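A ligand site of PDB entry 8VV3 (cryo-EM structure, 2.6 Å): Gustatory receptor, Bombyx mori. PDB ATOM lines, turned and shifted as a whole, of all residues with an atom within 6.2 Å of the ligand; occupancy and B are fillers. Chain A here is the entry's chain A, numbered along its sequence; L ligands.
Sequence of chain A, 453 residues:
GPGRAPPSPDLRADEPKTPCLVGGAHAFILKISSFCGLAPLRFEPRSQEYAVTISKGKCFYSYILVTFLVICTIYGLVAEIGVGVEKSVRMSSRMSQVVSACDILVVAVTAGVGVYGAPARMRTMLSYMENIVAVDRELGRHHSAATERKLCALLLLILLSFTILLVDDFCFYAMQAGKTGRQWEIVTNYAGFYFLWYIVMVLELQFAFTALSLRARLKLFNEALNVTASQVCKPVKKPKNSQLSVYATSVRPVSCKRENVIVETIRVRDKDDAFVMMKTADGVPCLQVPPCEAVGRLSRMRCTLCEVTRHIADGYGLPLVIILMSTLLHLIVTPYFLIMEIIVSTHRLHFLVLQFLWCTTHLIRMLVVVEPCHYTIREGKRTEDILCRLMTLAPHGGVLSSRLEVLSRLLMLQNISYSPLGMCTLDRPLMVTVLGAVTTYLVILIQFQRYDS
The side-chain carboxylate of Asp 169 lies within hydrogen-bond range of an oxygen (O1) of the ligand, at 2.6 Å. OD2 of Asp 103 lies within hydrogen-bond range of O3 of the ligand (2.7 Å). O4 of the ligand is in hydrogen-bond range of OG1 of Thr 334. The side-chain amide nitrogen of Gln 355 is in hydrogen-bond range of an oxygen (O5) of the ligand. NE2 of His 362 sits at hydrogen-bond distance from O4 of the ligand, 2.9 Å away. The guanidinium group of Arg 90 sits at hydrogen-bond distance from an oxygen (O2) of the ligand, at 3.0 Å. O1 of the ligand lies within hydrogen-bond range of OH of Tyr 194, 3.0 Å away. An oxygen (O3) of the ligand lies close to the indole nitrogen (NE1) of Trp 197 (3.5 Å).
OD2 of Asp 169 sits close to OH of Tyr 194, 3.5 Å away. The indole nitrogen of Trp 358 sits at hydrogen-bond distance from the side-chain carboxylate of Asp 169, at 2.8 Å. The side-chain hydroxyl (OG1) of Thr 334 sits at hydrogen-bond distance from a ring nitrogen (NE2) of His 362, 3.5 Å away. OG1 of Thr 334 is in hydrogen-bond range of O of His 330, 3.0 Å away. The backbone carbonyl oxygen (O) of Trp 358 lies close to a ring nitrogen (NE2) of His 362, at 3.5 Å.
Phe 193 touches the ligand (CE2 to C1, 3.8 Å). CD2 of His 330 touches O4 of the ligand, at 3.8 Å. Trp 358 touches the ligand (CZ2 to C1, 3.5 Å). Hydrophobic or aromatic side chains within 4 Å of the ligand: Phe 193, Tyr 194, Trp 197, His 330, Trp 358 and His 362. Along chain A the residues within 4 Å of the ligand span positions 90 to 362.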
ATOM      1  N   ARG A  90      27.973  24.480  28.098  1.00  0.00           N
ATOM      2  CA  ARG A  90      27.056  24.332  26.970  1.00  0.00           C
ATOM      3  C   ARG A  90      27.766  24.579  25.647  1.00  0.00           C
ATOM      4  O   ARG A  90      27.574  23.840  24.678  1.00  0.00           O
ATOM      5  CB  ARG A  90      25.866  25.275  27.121  1.00  0.00           C
ATOM      6  CG  ARG A  90      24.973  24.961  28.310  1.00  0.00           C
ATOM      7  CD  ARG A  90      23.524  25.220  27.970  1.00  0.00           C
ATOM      8  NE  ARG A  90      23.177  24.722  26.642  1.00  0.00           N
ATOM      9  CZ  ARG A  90      22.003  24.915  26.057  1.00  0.00           C
ATOM     10  NH1 ARG A  90      21.041  25.605  26.641  1.00  0.00           N
ATOM     11  NH2 ARG A  90      21.791  24.411  24.847  1.00  0.00           N
ATOM     12  N   ASP A 103      20.961  29.710  17.960  1.00  0.00           N
ATOM     13  CA  ASP A 103      19.741  29.229  18.613  1.00  0.00           C
ATOM     14  C   ASP A 103      19.157  30.284  19.540  1.00  0.00           C
ATOM     15  O   ASP A 103      17.965  30.608  19.479  1.00  0.00           O
ATOM     16  CB  ASP A 103      20.047  27.936  19.377  1.00  0.00           C
ATOM     17  CG  ASP A 103      18.845  27.389  20.124  1.00  0.00           C
ATOM     18  OD1 ASP A 103      17.701  27.747  19.770  1.00  0.00           O
ATOM     19  OD2 ASP A 103      19.045  26.596  21.059  1.00  0.00           O
ATOM     20  N   VAL A 107      15.577  32.325  18.890  1.00  0.00           N
ATOM     21  CA  VAL A 107      14.500  32.255  19.881  1.00  0.00           C
ATOM     22  C   VAL A 107      14.147  33.656  20.379  1.00  0.00           C
ATOM     23  O   VAL A 107      12.964  33.998  20.517  1.00  0.00           O
ATOM     24  CB  VAL A 107      14.896  31.324  21.034  1.00  0.00           C
ATOM     25  CG1 VAL A 107      13.943  31.476  22.213  1.00  0.00           C
ATOM     26  CG2 VAL A 107      14.927  29.885  20.561  1.00  0.00           C
ATOM     27  N   LEU A 166      11.580  22.257  29.323  1.00  0.00           N
ATOM     28  CA  LEU A 166      12.401  23.424  29.603  1.00  0.00           C
ATOM     29  C   LEU A 166      13.020  23.339  30.989  1.00  0.00           C
ATOM     30  O   LEU A 166      14.221  23.607  31.175  1.00  0.00           O
ATOM     31  CB  LEU A 166      11.566  24.707  29.485  1.00  0.00           C
ATOM     32  CG  LEU A 166      11.096  25.181  28.116  1.00  0.00           C
ATOM     33  CD1 LEU A 166      10.502  26.563  28.255  1.00  0.00           C
ATOM     34  CD2 LEU A 166      12.234  25.187  27.113  1.00  0.00           C
ATOM     35  N   ASP A 169      15.722  20.588  31.088  1.00  0.00           N
ATOM     36  CA  ASP A 169      16.939  20.966  30.385  1.00  0.00           C
ATOM     37  C   ASP A 169      17.710  22.015  31.167  1.00  0.00           C
ATOM     38  O   ASP A 169      18.947  21.951  31.283  1.00  0.00           O
ATOM     39  CB  ASP A 169      16.573  21.476  28.991  1.00  0.00           C
ATOM     40  CG  ASP A 169      17.767  21.540  28.072  1.00  0.00           C
ATOM     41  OD1 ASP A 169      18.860  21.170  28.511  1.00  0.00           O
ATOM     42  OD2 ASP A 169      17.597  21.957  26.907  1.00  0.00           O
ATOM     43  N   PHE A 170      16.996  22.995  31.742  1.00  0.00           N
ATOM     44  CA  PHE A 170      17.631  24.020  32.560  1.00  0.00           C
ATOM     45  C   PHE A 170      18.305  23.412  33.778  1.00  0.00           C
ATOM     46  O   PHE A 170      19.462  23.735  34.088  1.00  0.00           O
ATOM     47  CB  PHE A 170      16.575  25.048  32.988  1.00  0.00           C
ATOM     48  CG  PHE A 170      17.124  26.167  33.816  1.00  0.00           C
ATOM     49  CD1 PHE A 170      17.910  27.158  33.242  1.00  0.00           C
ATOM     50  CD2 PHE A 170      16.838  26.252  35.163  1.00  0.00           C
ATOM     51  CE1 PHE A 170      18.404  28.188  33.993  1.00  0.00           C
ATOM     52  CE2 PHE A 170      17.338  27.281  35.926  1.00  0.00           C
ATOM     53  CZ  PHE A 170      18.117  28.260  35.332  1.00  0.00           C
ATOM     54  N   TYR A 173      21.500  21.408  32.699  1.00  0.00           N
ATOM     55  CA  TYR A 173      22.669  22.236  32.384  1.00  0.00           C
ATOM     56  C   TYR A 173      23.163  23.009  33.598  1.00  0.00           C
ATOM     57  O   TYR A 173      24.348  23.359  33.665  1.00  0.00           O
ATOM     58  CB  TYR A 173      22.349  23.175  31.237  1.00  0.00           C
ATOM     59  CG  TYR A 173      22.510  22.523  29.878  1.00  0.00           C
ATOM     60  CD1 TYR A 173      23.690  21.873  29.539  1.00  0.00           C
ATOM     61  CD2 TYR A 173      21.483  22.548  28.947  1.00  0.00           C
ATOM     62  CE1 TYR A 173      23.837  21.279  28.311  1.00  0.00           C
ATOM     63  CE2 TYR A 173      21.631  21.954  27.719  1.00  0.00           C
ATOM     64  CZ  TYR A 173      22.809  21.318  27.397  1.00  0.00           C
ATOM     65  OH  TYR A 173      22.947  20.726  26.167  1.00  0.00           O
ATOM     66  N   PHE A 193      16.637  32.992  28.338  1.00  0.00           N
ATOM     67  CA  PHE A 193      16.505  32.108  27.186  1.00  0.00           C
ATOM     68  C   PHE A 193      15.334  31.150  27.352  1.00  0.00           C
ATOM     69  O   PHE A 193      14.530  30.974  26.427  1.00  0.00           O
ATOM     70  CB  PHE A 193      17.810  31.333  26.991  1.00  0.00           C
ATOM     71  CG  PHE A 193      17.804  30.421  25.791  1.00  0.00           C
ATOM     72  CD1 PHE A 193      17.424  30.896  24.551  1.00  0.00           C
ATOM     73  CD2 PHE A 193      18.179  29.101  25.923  1.00  0.00           C
ATOM     74  CE1 PHE A 193      17.416  30.055  23.460  1.00  0.00           C
ATOM     75  CE2 PHE A 193      18.185  28.265  24.825  1.00  0.00           C
ATOM     76  CZ  PHE A 193      17.804  28.742  23.593  1.00  0.00           C
ATOM     77  N   TYR A 194      15.206  30.536  28.524  1.00  0.00           N
ATOM     78  CA  TYR A 194      14.107  29.589  28.715  1.00  0.00           C
ATOM     79  C   TYR A 194      12.765  30.301  28.831  1.00  0.00           C
ATOM     80  O   TYR A 194      11.735  29.774  28.379  1.00  0.00           O
ATOM     81  CB  TYR A 194      14.400  28.714  29.936  1.00  0.00           C
ATOM     82  CG  TYR A 194      15.438  27.649  29.639  1.00  0.00           C
ATOM     83  CD1 TYR A 194      15.138  26.576  28.819  1.00  0.00           C
ATOM     84  CD2 TYR A 194      16.713  27.743  30.159  1.00  0.00           C
ATOM     85  CE1 TYR A 194      16.078  25.610  28.539  1.00  0.00           C
ATOM     86  CE2 TYR A 194      17.667  26.784  29.881  1.00  0.00           C
ATOM     87  CZ  TYR A 194      17.343  25.720  29.074  1.00  0.00           C
ATOM     88  OH  TYR A 194      18.297  24.761  28.795  1.00  0.00           O
ATOM     89  N   TRP A 197      11.779  30.836  25.337  1.00  0.00           N
ATOM     90  CA  TRP A 197      11.230  29.582  24.805  1.00  0.00           C
ATOM     91  C   TRP A 197       9.762  29.417  25.185  1.00  0.00           C
ATOM     92  O   TRP A 197       8.921  29.054  24.349  1.00  0.00           O
ATOM     93  CB  TRP A 197      12.019  28.376  25.317  1.00  0.00           C
ATOM     94  CG  TRP A 197      13.083  27.877  24.406  1.00  0.00           C
ATOM     95  CD1 TRP A 197      14.417  27.782  24.669  1.00  0.00           C
ATOM     96  CD2 TRP A 197      12.901  27.405  23.059  1.00  0.00           C
ATOM     97  NE1 TRP A 197      15.075  27.263  23.579  1.00  0.00           N
ATOM     98  CE2 TRP A 197      14.171  27.034  22.579  1.00  0.00           C
ATOM     99  CE3 TRP A 197      11.789  27.271  22.218  1.00  0.00           C
ATOM    100  CZ2 TRP A 197      14.349  26.527  21.296  1.00  0.00           C
ATOM    101  CZ3 TRP A 197      11.973  26.766  20.957  1.00  0.00           C
ATOM    102  CH2 TRP A 197      13.247  26.396  20.500  1.00  0.00           C
ATOM    103  N   HIS A 330      16.544  24.678  13.946  1.00  0.00           N
ATOM    104  CA  HIS A 330      16.646  23.731  15.053  1.00  0.00           C
ATOM    105  C   HIS A 330      16.606  22.292  14.563  1.00  0.00           C
ATOM    106  O   HIS A 330      17.349  21.453  15.071  1.00  0.00           O
ATOM    107  CB  HIS A 330      15.523  24.008  16.056  1.00  0.00           C
ATOM    108  CG  HIS A 330      15.722  25.260  16.841  1.00  0.00           C
ATOM    109  ND1 HIS A 330      14.875  26.338  16.747  1.00  0.00           N
ATOM    110  CD2 HIS A 330      16.674  25.616  17.737  1.00  0.00           C
ATOM    111  CE1 HIS A 330      15.287  27.298  17.558  1.00  0.00           C
ATOM    112  NE2 HIS A 330      16.382  26.890  18.165  1.00  0.00           N
ATOM    113  N   VAL A 333      20.149  21.720  13.501  1.00  0.00           N
ATOM    114  CA  VAL A 333      21.259  21.702  14.451  1.00  0.00           C
ATOM    115  C   VAL A 333      21.086  20.616  15.514  1.00  0.00           C
ATOM    116  O   VAL A 333      22.050  19.949  15.886  1.00  0.00           O
ATOM    117  CB  VAL A 333      21.466  23.088  15.090  1.00  0.00           C
ATOM    118  CG1 VAL A 333      21.889  24.102  14.031  1.00  0.00           C
ATOM    119  CG2 VAL A 333      20.213  23.556  15.814  1.00  0.00           C
ATOM    120  N   THR A 334      19.873  20.432  16.034  1.00  0.00           N
ATOM    121  CA  THR A 334      19.673  19.453  17.107  1.00  0.00           C
ATOM    122  C   THR A 334      19.967  18.028  16.673  1.00  0.00           C
ATOM    123  O   THR A 334      20.721  17.334  17.382  1.00  0.00           O
ATOM    124  CB  THR A 334      18.244  19.593  17.677  1.00  0.00           C
ATOM    125  OG1 THR A 334      17.968  20.975  17.945  1.00  0.00           O
ATOM    126  CG2 THR A 334      18.096  18.788  18.953  1.00  0.00           C
ATOM    127  N   PHE A 337      24.004  17.507  16.300  1.00  0.00           N
ATOM    128  CA  PHE A 337      24.787  17.278  17.517  1.00  0.00           C
ATOM    129  C   PHE A 337      24.301  16.044  18.264  1.00  0.00           C
ATOM    130  O   PHE A 337      25.094  15.424  18.985  1.00  0.00           O
ATOM    131  CB  PHE A 337      24.745  18.519  18.404  1.00  0.00           C
ATOM    132  CG  PHE A 337      25.483  19.685  17.830  1.00  0.00           C
ATOM    133  CD1 PHE A 337      26.864  19.761  17.926  1.00  0.00           C
ATOM    134  CD2 PHE A 337      24.816  20.699  17.172  1.00  0.00           C
ATOM    135  CE1 PHE A 337      27.561  20.819  17.388  1.00  0.00           C
ATOM    136  CE2 PHE A 337      25.506  21.769  16.630  1.00  0.00           C
ATOM    137  CZ  PHE A 337      26.876  21.831  16.748  1.00  0.00           C
ATOM    138  N   PHE A 351      21.784  13.662  28.184  1.00  0.00           N
ATOM    139  CA  PHE A 351      21.960  14.565  27.050  1.00  0.00           C
ATOM    140  C   PHE A 351      21.282  14.018  25.800  1.00  0.00           C
ATOM    141  O   PHE A 351      20.600  14.761  25.077  1.00  0.00           O
ATOM    142  CB  PHE A 351      23.452  14.793  26.787  1.00  0.00           C
ATOM    143  CG  PHE A 351      23.720  15.750  25.652  1.00  0.00           C
ATOM    144  CD1 PHE A 351      23.595  17.111  25.835  1.00  0.00           C
ATOM    145  CD2 PHE A 351      24.090  15.271  24.409  1.00  0.00           C
ATOM    146  CE1 PHE A 351      23.840  17.985  24.799  1.00  0.00           C
ATOM    147  CE2 PHE A 351      24.335  16.133  23.365  1.00  0.00           C
ATOM    148  CZ  PHE A 351      24.207  17.496  23.557  1.00  0.00           C
ATOM    149  N   LEU A 354      17.504  14.322  26.151  1.00  0.00           N
ATOM    150  CA  LEU A 354      17.073  15.701  25.938  1.00  0.00           C
ATOM    151  C   LEU A 354      17.152  16.081  24.462  1.00  0.00           C
ATOM    152  O   LEU A 354      16.299  16.810  23.964  1.00  0.00           O
ATOM    153  CB  LEU A 354      17.916  16.651  26.783  1.00  0.00           C
ATOM    154  CG  LEU A 354      17.536  16.775  28.256  1.00  0.00           C
ATOM    155  CD1 LEU A 354      18.546  17.633  29.005  1.00  0.00           C
ATOM    156  CD2 LEU A 354      16.133  17.341  28.403  1.00  0.00           C
ATOM    157  N   GLN A 355      18.170  15.597  23.747  1.00  0.00           N
ATOM    158  CA  GLN A 355      18.301  15.928  22.337  1.00  0.00           C
ATOM    159  C   GLN A 355      17.183  15.298  21.519  1.00  0.00           C
ATOM    160  O   GLN A 355      16.616  15.941  20.614  1.00  0.00           O
ATOM    161  CB  GLN A 355      19.663  15.486  21.813  1.00  0.00           C
ATOM    162  CG  GLN A 355      20.829  16.292  22.358  1.00  0.00           C
ATOM    163  CD  GLN A 355      20.514  17.754  22.513  1.00  0.00           C
ATOM    164  OE1 GLN A 355      20.206  18.222  23.616  1.00  0.00           O
ATOM    165  NE2 GLN A 355      20.579  18.496  21.412  1.00  0.00           N
ATOM    166  N   TRP A 358      14.078  17.244  22.222  1.00  0.00           N
ATOM    167  CA  TRP A 358      14.073  18.534  21.532  1.00  0.00           C
ATOM    168  C   TRP A 358      13.795  18.371  20.046  1.00  0.00           C
ATOM    169  O   TRP A 358      13.130  19.222  19.438  1.00  0.00           O
ATOM    170  CB  TRP A 358      15.391  19.260  21.764  1.00  0.00           C
ATOM    171  CG  TRP A 358      15.380  20.108  22.995  1.00  0.00           C
ATOM    172  CD1 TRP A 358      16.061  19.883  24.155  1.00  0.00           C
ATOM    173  CD2 TRP A 358      14.656  21.318  23.185  1.00  0.00           C
ATOM    174  NE1 TRP A 358      15.803  20.879  25.059  1.00  0.00           N
ATOM    175  CE2 TRP A 358      14.937  21.781  24.485  1.00  0.00           C
ATOM    176  CE3 TRP A 358      13.784  22.069  22.382  1.00  0.00           C
ATOM    177  CZ2 TRP A 358      14.383  22.953  25.000  1.00  0.00           C
ATOM    178  CZ3 TRP A 358      13.237  23.229  22.902  1.00  0.00           C
ATOM    179  CH2 TRP A 358      13.540  23.651  24.195  1.00  0.00           C
ATOM    180  N   HIS A 362      10.684  20.235  18.252  1.00  0.00           N
ATOM    181  CA  HIS A 362      10.704  21.051  17.048  1.00  0.00           C
ATOM    182  C   HIS A 362       9.752  20.508  15.985  1.00  0.00           C
ATOM    183  O   HIS A 362       9.068  21.278  15.296  1.00  0.00           O
ATOM    184  CB  HIS A 362      12.128  21.139  16.496  1.00  0.00           C
ATOM    185  CG  HIS A 362      13.120  21.699  17.481  1.00  0.00           C
ATOM    186  ND1 HIS A 362      12.827  22.777  18.293  1.00  0.00           N
ATOM    187  CD2 HIS A 362      14.385  21.324  17.783  1.00  0.00           C
ATOM    188  CE1 HIS A 362      13.884  23.044  19.046  1.00  0.00           C
ATOM    189  NE2 HIS A 362      14.830  22.173  18.766  1.00  0.00           N
HETATM  190  C1  LIG L   1      17.513  24.571  24.582  1.00  0.00           C
HETATM  191  O1  LIG L   1      18.139  24.282  25.828  1.00  0.00           O
HETATM  192  C2  LIG L   1      18.304  23.906  23.454  1.00  0.00           C
HETATM  193  O2  LIG L   1      19.401  24.741  23.099  1.00  0.00           O
HETATM  194  C3  LIG L   1      17.408  23.692  22.231  1.00  0.00           C
HETATM  195  O3  LIG L   1      16.964  24.958  21.747  1.00  0.00           O
HETATM  196  C4  LIG L   1      18.213  22.995  21.135  1.00  0.00           C
HETATM  197  O4  LIG L   1      17.349  22.696  20.046  1.00  0.00           O
HETATM  198  C5  LIG L   1      18.821  21.696  21.689  1.00  0.00           C
HETATM  199  O5  LIG L   1      19.675  21.126  20.691  1.00  0.00           O
HETATM  200  C6  LIG L   1      19.630  21.986  22.946  1.00  0.00           C
HETATM  201  O6  LIG L   1      18.800  22.639  23.909  1.00  0.00           O
